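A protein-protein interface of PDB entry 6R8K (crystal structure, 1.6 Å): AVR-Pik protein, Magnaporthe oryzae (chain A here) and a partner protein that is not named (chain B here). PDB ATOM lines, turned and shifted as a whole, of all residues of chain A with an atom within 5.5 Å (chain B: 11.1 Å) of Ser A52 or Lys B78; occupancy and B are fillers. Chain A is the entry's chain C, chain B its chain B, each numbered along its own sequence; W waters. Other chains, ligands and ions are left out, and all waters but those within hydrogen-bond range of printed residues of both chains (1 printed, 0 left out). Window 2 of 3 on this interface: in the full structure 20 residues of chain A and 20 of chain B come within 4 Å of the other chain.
The backbone carbonyl oxygen (O) of Gln B76 is in hydrogen-bond range of the indole nitrogen (NE1) of Trp A54.
The side-chain amino group (NZ) of Lys B78 lies within salt-bridge range of the side-chain carboxylate (OE2) of Glu A33, 2.8 Å away.
The side-chain amino group of Lys B78 lies within hydrogen-bond range of the backbone carbonyl oxygen of Ser A52 (2.9 Å).
The backbone carbonyl oxygen (O) of Lys B5 lies within hydrogen-bond range of the backbone NH (N) of Ala B77 (2.9 Å).
O of Pro A30 lies within hydrogen-bond range of OH of Tyr A51, at 2.6 Å.
N of Ser A52 lies within hydrogen-bond range of OE1 of Glu A33 (2.8 Å).
The side-chain sulfur of Cys A34 sits at hydrogen-bond distance from the backbone NH of Ser A52 (3.6 Å).
The backbone carbonyl oxygen of Tyr A51 sits at hydrogen-bond distance from the side-chain hydroxyl of Ser A69, 2.7 Å away.
SG of Cys A34 is disulfide-bonded to SG of Cys A73 (2.1 Å).
CG of Pro A30 touches O of Lys B78, 3.3 Å away.
CA of Ala B77 touches CE2 of Tyr A51, 3.8 Å away.
Lys B78 touches Tyr A51.
Trp A54 touches Leu B4.
Trp A54 touches Ala B77.
Lys B78 touches Trp A54.
Ser A52 touches just one residue of chain B: Lys B78.
Of chain A, only Pro A30, Glu A33, Tyr A51, Ser A52 and Trp A54 come within 4 Å of Lys B78.
Of chain B, only Lys B78 (3.3 Å) comes within 4 Å of Pro A30.
No residue of chain B comes within 4 Å of Cys A34.
No residue of chain B comes within 4 Å of Cys A50.
Tyr A51 touches just these residues of chain B: Ala B77 (3.8 Å) and Lys B78 (3.6 Å).
Ser A53 touches none of the printed residues of chain B.
No residue of chain B comes within 4 Å of Ser A69.
Of the printed residues of chain B, Trp A54 touches Leu B4, Gln B76, Ala B77 and Lys B78.
Of the printed residues of chain A, Gln B76 touches Trp A54 (2.9 Å).
The nearest residue of chain B that does not touch Ser A52 is Asp B80 (6.3 Å).
Of the 14 printed residues of chain A, 5 touch a printed residue of chain B.
Hydrophobic or aromatic side chains of chain A within 4 Å of the printed part of chain B: Pro A30, Tyr A51 and Trp A54.
Among the printed residues, Asp or Glu carboxylates within 4 Å of a Lys or Arg side-chain nitrogen of the other chain: Glu A33 with Lys B78 (2.8 Å).
Water W1 lies within hydrogen-bond range of NZ of Lys B7 and OH of Tyr A51.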
ATOM      1  N   PRO A  30     -20.895  -6.538  -3.177  1.00  0.00           N
ATOM      2  CA  PRO A  30     -21.822  -7.360  -3.930  1.00  0.00           C
ATOM      3  C   PRO A  30     -22.724  -6.474  -4.787  1.00  0.00           C
ATOM      4  O   PRO A  30     -23.002  -5.330  -4.440  1.00  0.00           O
ATOM      5  CB  PRO A  30     -22.586  -8.125  -2.849  1.00  0.00           C
ATOM      6  CG  PRO A  30     -21.570  -8.219  -1.758  1.00  0.00           C
ATOM      7  CD  PRO A  30     -20.958  -6.835  -1.734  1.00  0.00           C
ATOM      8  N   GLU A  33     -29.483  -6.156  -5.625  1.00  0.00           N
ATOM      9  CA  GLU A  33     -30.473  -6.962  -6.394  1.00  0.00           C
ATOM     10  C   GLU A  33     -31.649  -6.123  -6.873  1.00  0.00           C
ATOM     11  O   GLU A  33     -32.461  -6.619  -7.678  1.00  0.00           O
ATOM     12  CB  GLU A  33     -31.008  -8.109  -5.539  1.00  0.00           C
ATOM     13  CG  GLU A  33     -29.886  -8.978  -5.004  1.00  0.00           C
ATOM     14  CD  GLU A  33     -29.368  -8.647  -3.615  1.00  0.00           C
ATOM     15  OE1 GLU A  33     -29.489  -7.445  -3.178  1.00  0.00           O
ATOM     16  OE2 GLU A  33     -28.755  -9.581  -2.968  1.00  0.00           O
ATOM     17  N   CYS A  34     -31.815  -4.915  -6.331  1.00  0.00           N
ATOM     18  CA  CYS A  34     -33.034  -4.108  -6.531  1.00  0.00           C
ATOM     19  C   CYS A  34     -32.779  -2.773  -7.243  1.00  0.00           C
ATOM     20  O   CYS A  34     -31.746  -2.178  -7.068  1.00  0.00           O
ATOM     21  CB  CYS A  34     -33.677  -3.740  -5.207  1.00  0.00           C
ATOM     22  SG  CYS A  34     -33.940  -5.144  -4.079  1.00  0.00           S
ATOM     23  N   CYS A  50     -30.457  -0.803  -4.723  1.00  0.00           N
ATOM     24  CA  CYS A  50     -30.323  -1.153  -3.292  1.00  0.00           C
ATOM     25  C   CYS A  50     -30.328  -2.669  -3.155  1.00  0.00           C
ATOM     26  O   CYS A  50     -30.779  -3.385  -4.089  1.00  0.00           O
ATOM     27  CB  CYS A  50     -31.418  -0.509  -2.432  1.00  0.00           C
ATOM     28  SG  CYS A  50     -33.122  -0.950  -2.845  1.00  0.00           S
ATOM     29  N   TYR A  51     -29.898  -3.141  -1.993  1.00  0.00           N
ATOM     30  CA  TYR A  51     -29.891  -4.590  -1.699  1.00  0.00           C
ATOM     31  C   TYR A  51     -31.283  -5.068  -1.321  1.00  0.00           C
ATOM     32  O   TYR A  51     -32.042  -4.306  -0.686  1.00  0.00           O
ATOM     33  CB  TYR A  51     -28.923  -4.946  -0.579  1.00  0.00           C
ATOM     34  CG  TYR A  51     -27.494  -4.734  -0.988  1.00  0.00           C
ATOM     35  CD1 TYR A  51     -26.869  -5.612  -1.871  1.00  0.00           C
ATOM     36  CD2 TYR A  51     -26.804  -3.604  -0.607  1.00  0.00           C
ATOM     37  CE1 TYR A  51     -25.555  -5.425  -2.264  1.00  0.00           C
ATOM     38  CE2 TYR A  51     -25.512  -3.374  -1.036  1.00  0.00           C
ATOM     39  CZ  TYR A  51     -24.880  -4.283  -1.870  1.00  0.00           C
ATOM     40  OH  TYR A  51     -23.614  -4.016  -2.283  1.00  0.00           O
ATOM     41  N   SER A  52     -31.565  -6.340  -1.630  1.00  0.00           N
ATOM     42  CA  SER A  52     -32.770  -7.067  -1.159  1.00  0.00           C
ATOM     43  C   SER A  52     -32.510  -7.535   0.278  1.00  0.00           C
ATOM     44  O   SER A  52     -31.343  -7.626   0.678  1.00  0.00           O
ATOM     45  CB  SER A  52     -33.098  -8.228  -2.067  1.00  0.00           C
ATOM     46  OG  SER A  52     -32.001  -9.094  -2.139  1.00  0.00           O
ATOM     47  N   SER A  53     -33.575  -7.825   0.991  1.00  0.00           N
ATOM     48  CA  SER A  53     -33.550  -8.384   2.373  1.00  0.00           C
ATOM     49  C   SER A  53     -32.644  -7.502   3.234  1.00  0.00           C
ATOM     50  O   SER A  53     -31.713  -8.011   3.900  1.00  0.00           O
ATOM     51  CB  SER A  53     -33.143  -9.822   2.375  1.00  0.00           C
ATOM     52  OG  SER A  53     -34.086 -10.570   1.650  1.00  0.00           O
ATOM     53  N   TRP A  54     -32.817  -6.177   3.127  1.00  0.00           N
ATOM     54  CA  TRP A  54     -31.805  -5.244   3.672  1.00  0.00           C
ATOM     55  C   TRP A  54     -32.486  -3.960   4.121  1.00  0.00           C
ATOM     56  O   TRP A  54     -33.722  -3.958   4.338  1.00  0.00           O
ATOM     57  CB  TRP A  54     -30.670  -5.015   2.674  1.00  0.00           C
ATOM     58  CG  TRP A  54     -29.344  -4.627   3.260  1.00  0.00           C
ATOM     59  CD1 TRP A  54     -28.619  -3.539   2.899  1.00  0.00           C
ATOM     60  CD2 TRP A  54     -28.573  -5.278   4.290  1.00  0.00           C
ATOM     61  NE1 TRP A  54     -27.461  -3.471   3.607  1.00  0.00           N
ATOM     62  CE2 TRP A  54     -27.401  -4.520   4.473  1.00  0.00           C
ATOM     63  CE3 TRP A  54     -28.763  -6.427   5.066  1.00  0.00           C
ATOM     64  CZ2 TRP A  54     -26.424  -4.846   5.405  1.00  0.00           C
ATOM     65  CZ3 TRP A  54     -27.782  -6.770   5.969  1.00  0.00           C
ATOM     66  CH2 TRP A  54     -26.635  -5.997   6.129  1.00  0.00           C
ATOM     67  N   SER A  69     -36.112  -3.449   2.693  1.00  0.00           N
ATOM     68  CA  SER A  69     -36.415  -4.258   1.500  1.00  0.00           C
ATOM     69  C   SER A  69     -36.627  -5.704   1.918  1.00  0.00           C
ATOM     70  O   SER A  69     -35.848  -6.199   2.742  1.00  0.00           O
ATOM     71  CB  SER A  69     -35.305  -4.166   0.490  1.00  0.00           C
ATOM     72  OG  SER A  69     -34.059  -4.524   1.051  1.00  0.00           O
ATOM     73  N   ASP A  70     -37.651  -6.326   1.342  1.00  0.00           N
ATOM     74  CA  ASP A  70     -37.918  -7.780   1.526  1.00  0.00           C
ATOM     75  C   ASP A  70     -37.094  -8.536   0.481  1.00  0.00           C
ATOM     76  O   ASP A  70     -36.302  -7.934  -0.266  1.00  0.00           O
ATOM     77  CB  ASP A  70     -39.429  -8.019   1.535  1.00  0.00           C
ATOM     78  CG  ASP A  70     -40.126  -8.098   0.202  1.00  0.00           C
ATOM     79  OD1 ASP A  70     -39.455  -7.926  -0.824  1.00  0.00           O
ATOM     80  OD2 ASP A  70     -41.376  -8.219   0.204  1.00  0.00           O
ATOM     81  N   ASP A  71     -37.250  -9.851   0.413  1.00  0.00           N
ATOM     82  CA  ASP A  71     -36.420 -10.672  -0.499  1.00  0.00           C
ATOM     83  C   ASP A  71     -36.846 -10.459  -1.958  1.00  0.00           C
ATOM     84  O   ASP A  71     -36.097 -10.915  -2.825  1.00  0.00           O
ATOM     85  CB  ASP A  71     -36.542 -12.145  -0.104  1.00  0.00           C
ATOM     86  CG  ASP A  71     -37.905 -12.724  -0.442  1.00  0.00           C
ATOM     87  OD1 ASP A  71     -38.930 -12.070  -0.157  1.00  0.00           O
ATOM     88  OD2 ASP A  71     -37.933 -13.844  -0.993  1.00  0.00           O
ATOM     89  N   ASN A  72     -37.999  -9.833  -2.223  1.00  0.00           N
ATOM     90  CA  ASN A  72     -38.491  -9.563  -3.598  1.00  0.00           C
ATOM     91  C   ASN A  72     -38.411  -8.073  -3.922  1.00  0.00           C
ATOM     92  O   ASN A  72     -39.035  -7.676  -4.902  1.00  0.00           O
ATOM     93  CB  ASN A  72     -39.890 -10.129  -3.824  1.00  0.00           C
ATOM     94  CG  ASN A  72     -39.844 -11.641  -3.838  1.00  0.00           C
ATOM     95  OD1 ASN A  72     -40.353 -12.293  -2.932  1.00  0.00           O
ATOM     96  ND2 ASN A  72     -39.154 -12.197  -4.815  1.00  0.00           N
ATOM     97  N   CYS A  73     -37.629  -7.305  -3.148  1.00  0.00           N
ATOM     98  CA  CYS A  73     -37.351  -5.859  -3.412  1.00  0.00           C
ATOM     99  C   CYS A  73     -38.596  -4.993  -3.157  1.00  0.00           C
ATOM    100  O   CYS A  73     -38.658  -3.866  -3.636  1.00  0.00           O
ATOM    101  CB  CYS A  73     -36.816  -5.639  -4.820  1.00  0.00           C
ATOM    102  SG  CYS A  73     -35.204  -6.402  -5.093  1.00  0.00           S
ATOM    103  N   LYS A  89     -37.293  -5.913  -8.478  1.00  0.00           N
ATOM    104  CA  LYS A  89     -36.128  -6.786  -8.647  1.00  0.00           C
ATOM    105  C   LYS A  89     -35.457  -6.399  -9.956  1.00  0.00           C
ATOM    106  O   LYS A  89     -36.148  -6.191 -10.939  1.00  0.00           O
ATOM    107  CB  LYS A  89     -36.510  -8.267  -8.729  1.00  0.00           C
ATOM    108  CG  LYS A  89     -36.349  -9.044  -7.440  1.00  0.00           C
ATOM    109  CD  LYS A  89     -34.927  -9.520  -7.155  1.00  0.00           C
ATOM    110  CE  LYS A  89     -34.885 -10.499  -5.988  1.00  0.00           C
ATOM    111  NZ  LYS A  89     -33.594 -10.489  -5.257  1.00  0.00           N
ATOM    112  N   LEU B   4     -19.068  -3.204   8.238  1.00  0.00           N
ATOM    113  CA  LEU B   4     -19.306  -3.360   6.780  1.00  0.00           C
ATOM    114  C   LEU B   4     -18.736  -2.152   6.010  1.00  0.00           C
ATOM    115  O   LEU B   4     -18.498  -1.074   6.590  1.00  0.00           O
ATOM    116  CB  LEU B   4     -20.813  -3.495   6.527  1.00  0.00           C
ATOM    117  CG  LEU B   4     -21.476  -4.781   7.032  1.00  0.00           C
ATOM    118  CD1 LEU B   4     -22.995  -4.650   7.024  1.00  0.00           C
ATOM    119  CD2 LEU B   4     -21.039  -5.987   6.206  1.00  0.00           C
ATOM    120  N   LYS B   5     -18.544  -2.325   4.706  1.00  0.00           N
ATOM    121  CA  LYS B   5     -18.361  -1.197   3.779  1.00  0.00           C
ATOM    122  C   LYS B   5     -19.612  -0.291   3.898  1.00  0.00           C
ATOM    123  O   LYS B   5     -20.691  -0.799   4.209  1.00  0.00           O
ATOM    124  CB  LYS B   5     -18.137  -1.755   2.364  1.00  0.00           C
ATOM    125  CG  LYS B   5     -16.709  -1.713   1.837  1.00  0.00           C
ATOM    126  CD  LYS B   5     -15.952  -3.023   1.896  1.00  0.00           C
ATOM    127  CE  LYS B   5     -16.134  -3.912   0.682  1.00  0.00           C
ATOM    128  NZ  LYS B   5     -16.942  -5.119   0.993  1.00  0.00           N
ATOM    129  N   GLN B   6     -19.450   1.009   3.694  1.00  0.00           N
ATOM    130  CA  GLN B   6     -20.597   1.938   3.588  1.00  0.00           C
ATOM    131  C   GLN B   6     -20.704   2.436   2.153  1.00  0.00           C
ATOM    132  O   GLN B   6     -19.725   2.472   1.432  1.00  0.00           O
ATOM    133  CB  GLN B   6     -20.494   3.100   4.569  1.00  0.00           C
ATOM    134  CG  GLN B   6     -20.606   2.633   6.015  1.00  0.00           C
ATOM    135  CD  GLN B   6     -21.555   3.471   6.821  1.00  0.00           C
ATOM    136  OE1 GLN B   6     -21.212   4.553   7.284  1.00  0.00           O
ATOM    137  NE2 GLN B   6     -22.764   2.961   6.984  1.00  0.00           N
ATOM    138  N   LYS B   7     -21.924   2.811   1.805  1.00  0.00           N
ATOM    139  CA  LYS B   7     -22.238   3.498   0.541  1.00  0.00           C
ATOM    140  C   LYS B   7     -22.851   4.824   0.946  1.00  0.00           C
ATOM    141  O   LYS B   7     -23.800   4.809   1.784  1.00  0.00           O
ATOM    142  CB  LYS B   7     -23.191   2.664  -0.313  1.00  0.00           C
ATOM    143  CG  LYS B   7     -23.606   3.304  -1.635  1.00  0.00           C
ATOM    144  CD  LYS B   7     -24.379   2.373  -2.572  1.00  0.00           C
ATOM    145  CE  LYS B   7     -25.145   1.273  -1.857  1.00  0.00           C
ATOM    146  NZ  LYS B   7     -26.115   0.565  -2.730  1.00  0.00           N
ATOM    147  N   VAL B  49     -18.174   4.501  -2.107  1.00  0.00           N
ATOM    148  CA  VAL B  49     -18.153   3.204  -1.375  1.00  0.00           C
ATOM    149  C   VAL B  49     -16.783   3.068  -0.710  1.00  0.00           C
ATOM    150  O   VAL B  49     -15.788   3.408  -1.364  1.00  0.00           O
ATOM    151  CB  VAL B  49     -18.434   2.033  -2.326  1.00  0.00           C
ATOM    152  CG1 VAL B  49     -18.185   0.692  -1.664  1.00  0.00           C
ATOM    153  CG2 VAL B  49     -19.856   2.115  -2.891  1.00  0.00           C
ATOM    154  N   GLY B  50     -16.776   2.622   0.545  1.00  0.00           N
ATOM    155  CA  GLY B  50     -15.524   2.365   1.280  1.00  0.00           C
ATOM    156  C   GLY B  50     -15.740   2.010   2.728  1.00  0.00           C
ATOM    157  O   GLY B  50     -16.855   2.145   3.251  1.00  0.00           O
ATOM    158  N   GLN B  73     -27.977   9.691   1.114  1.00  0.00           N
ATOM    159  CA  GLN B  73     -28.069   8.272   1.528  1.00  0.00           C
ATOM    160  C   GLN B  73     -26.835   7.874   2.307  1.00  0.00           C
ATOM    161  O   GLN B  73     -25.750   8.283   1.936  1.00  0.00           O
ATOM    162  CB  GLN B  73     -28.232   7.338   0.329  1.00  0.00           C
ATOM    163  CG  GLN B  73     -28.398   5.867   0.716  1.00  0.00           C
ATOM    164  CD  GLN B  73     -28.471   4.979  -0.504  1.00  0.00           C
ATOM    165  OE1 GLN B  73     -28.917   5.387  -1.589  1.00  0.00           O
ATOM    166  NE2 GLN B  73     -28.029   3.746  -0.307  1.00  0.00           N
ATOM    167  N   VAL B  74     -27.069   7.064   3.329  1.00  0.00           N
ATOM    168  CA  VAL B  74     -26.012   6.305   4.030  1.00  0.00           C
ATOM    169  C   VAL B  74     -26.553   4.899   4.198  1.00  0.00           C
ATOM    170  O   VAL B  74     -27.652   4.713   4.729  1.00  0.00           O
ATOM    171  CB  VAL B  74     -25.618   6.919   5.382  1.00  0.00           C
ATOM    172  CG1 VAL B  74     -24.470   6.119   5.991  1.00  0.00           C
ATOM    173  CG2 VAL B  74     -25.272   8.388   5.244  1.00  0.00           C
ATOM    174  N   SER B  75     -25.804   3.922   3.709  1.00  0.00           N
ATOM    175  CA  SER B  75     -26.177   2.498   3.868  1.00  0.00           C
ATOM    176  C   SER B  75     -24.919   1.667   3.982  1.00  0.00           C
ATOM    177  O   SER B  75     -23.839   2.210   3.763  1.00  0.00           O
ATOM    178  CB  SER B  75     -27.005   2.009   2.743  1.00  0.00           C
ATOM    179  OG  SER B  75     -26.366   2.248   1.498  1.00  0.00           O
ATOM    180  N   GLN B  76     -25.112   0.432   4.425  1.00  0.00           N
ATOM    181  CA  GLN B  76     -24.029  -0.561   4.570  1.00  0.00           C
ATOM    182  C   GLN B  76     -24.148  -1.525   3.400  1.00  0.00           C
ATOM    183  O   GLN B  76     -25.261  -1.782   2.931  1.00  0.00           O
ATOM    184  CB  GLN B  76     -24.160  -1.293   5.900  1.00  0.00           C
ATOM    185  CG  GLN B  76     -24.017  -0.364   7.092  1.00  0.00           C
ATOM    186  CD  GLN B  76     -23.988  -1.138   8.387  1.00  0.00           C
ATOM    187  OE1 GLN B  76     -24.885  -1.933   8.664  1.00  0.00           O
ATOM    188  NE2 GLN B  76     -22.948  -0.911   9.179  1.00  0.00           N
ATOM    189  N   ALA B  77     -23.025  -2.004   2.919  1.00  0.00           N
ATOM    190  CA  ALA B  77     -22.999  -3.029   1.859  1.00  0.00           C
ATOM    191  C   ALA B  77     -23.397  -4.355   2.497  1.00  0.00           C
ATOM    192  O   ALA B  77     -22.896  -4.692   3.563  1.00  0.00           O
ATOM    193  CB  ALA B  77     -21.661  -3.115   1.188  1.00  0.00           C
ATOM    194  N   LYS B  78     -24.352  -5.034   1.886  1.00  0.00           N
ATOM    195  CA  LYS B  78     -24.821  -6.334   2.386  1.00  0.00           C
ATOM    196  C   LYS B  78     -23.793  -7.418   2.042  1.00  0.00           C
ATOM    197  O   LYS B  78     -23.540  -7.647   0.834  1.00  0.00           O
ATOM    198  CB  LYS B  78     -26.178  -6.691   1.794  1.00  0.00           C
ATOM    199  CG  LYS B  78     -26.733  -8.000   2.333  1.00  0.00           C
ATOM    200  CD  LYS B  78     -28.079  -8.399   1.789  1.00  0.00           C
ATOM    201  CE  LYS B  78     -27.991  -8.783   0.322  1.00  0.00           C
ATOM    202  NZ  LYS B  78     -29.264  -9.381  -0.171  1.00  0.00           N
ATOM    203  N   GLU B  79     -23.287  -8.092   3.069  1.00  0.00           N
ATOM    204  CA  GLU B  79     -22.462  -9.329   2.940  1.00  0.00           C
ATOM    205  C   GLU B  79     -23.217 -10.463   3.648  1.00  0.00           C
ATOM    206  O   GLU B  79     -23.462 -10.341   4.868  1.00  0.00           O
ATOM    207  CB  GLU B  79     -21.078  -9.133   3.558  1.00  0.00           C
ATOM    208  CG  GLU B  79     -20.388  -7.863   3.111  1.00  0.00           C
ATOM    209  CD  GLU B  79     -19.169  -7.479   3.940  1.00  0.00           C
ATOM    210  OE1 GLU B  79     -19.029  -7.986   5.094  1.00  0.00           O
ATOM    211  OE2 GLU B  79     -18.360  -6.656   3.438  1.00  0.00           O
ATOM    212  N   ASP B  80     -23.594 -11.510   2.916  1.00  0.00           N
ATOM    213  CA  ASP B  80     -24.469 -12.604   3.423  1.00  0.00           C
ATOM    214  C   ASP B  80     -23.679 -13.489   4.399  1.00  0.00           C
ATOM    215  O   ASP B  80     -22.661 -13.041   4.942  1.00  0.00           O
ATOM    216  CB  ASP B  80     -25.077 -13.379   2.251  1.00  0.00           C
ATOM    217  CG  ASP B  80     -26.143 -12.584   1.514  1.00  0.00           C
ATOM    218  OD1 ASP B  80     -26.874 -11.831   2.186  1.00  0.00           O
ATOM    219  OD2 ASP B  80     -26.234 -12.725   0.281  1.00  0.00           O
ATOM    220  OXT ASP B  80     -24.040 -14.654   4.679  1.00  0.00           O
HETATM  221  O   HOH W   1     -24.478  -1.397  -3.787  1.00  0.00           O
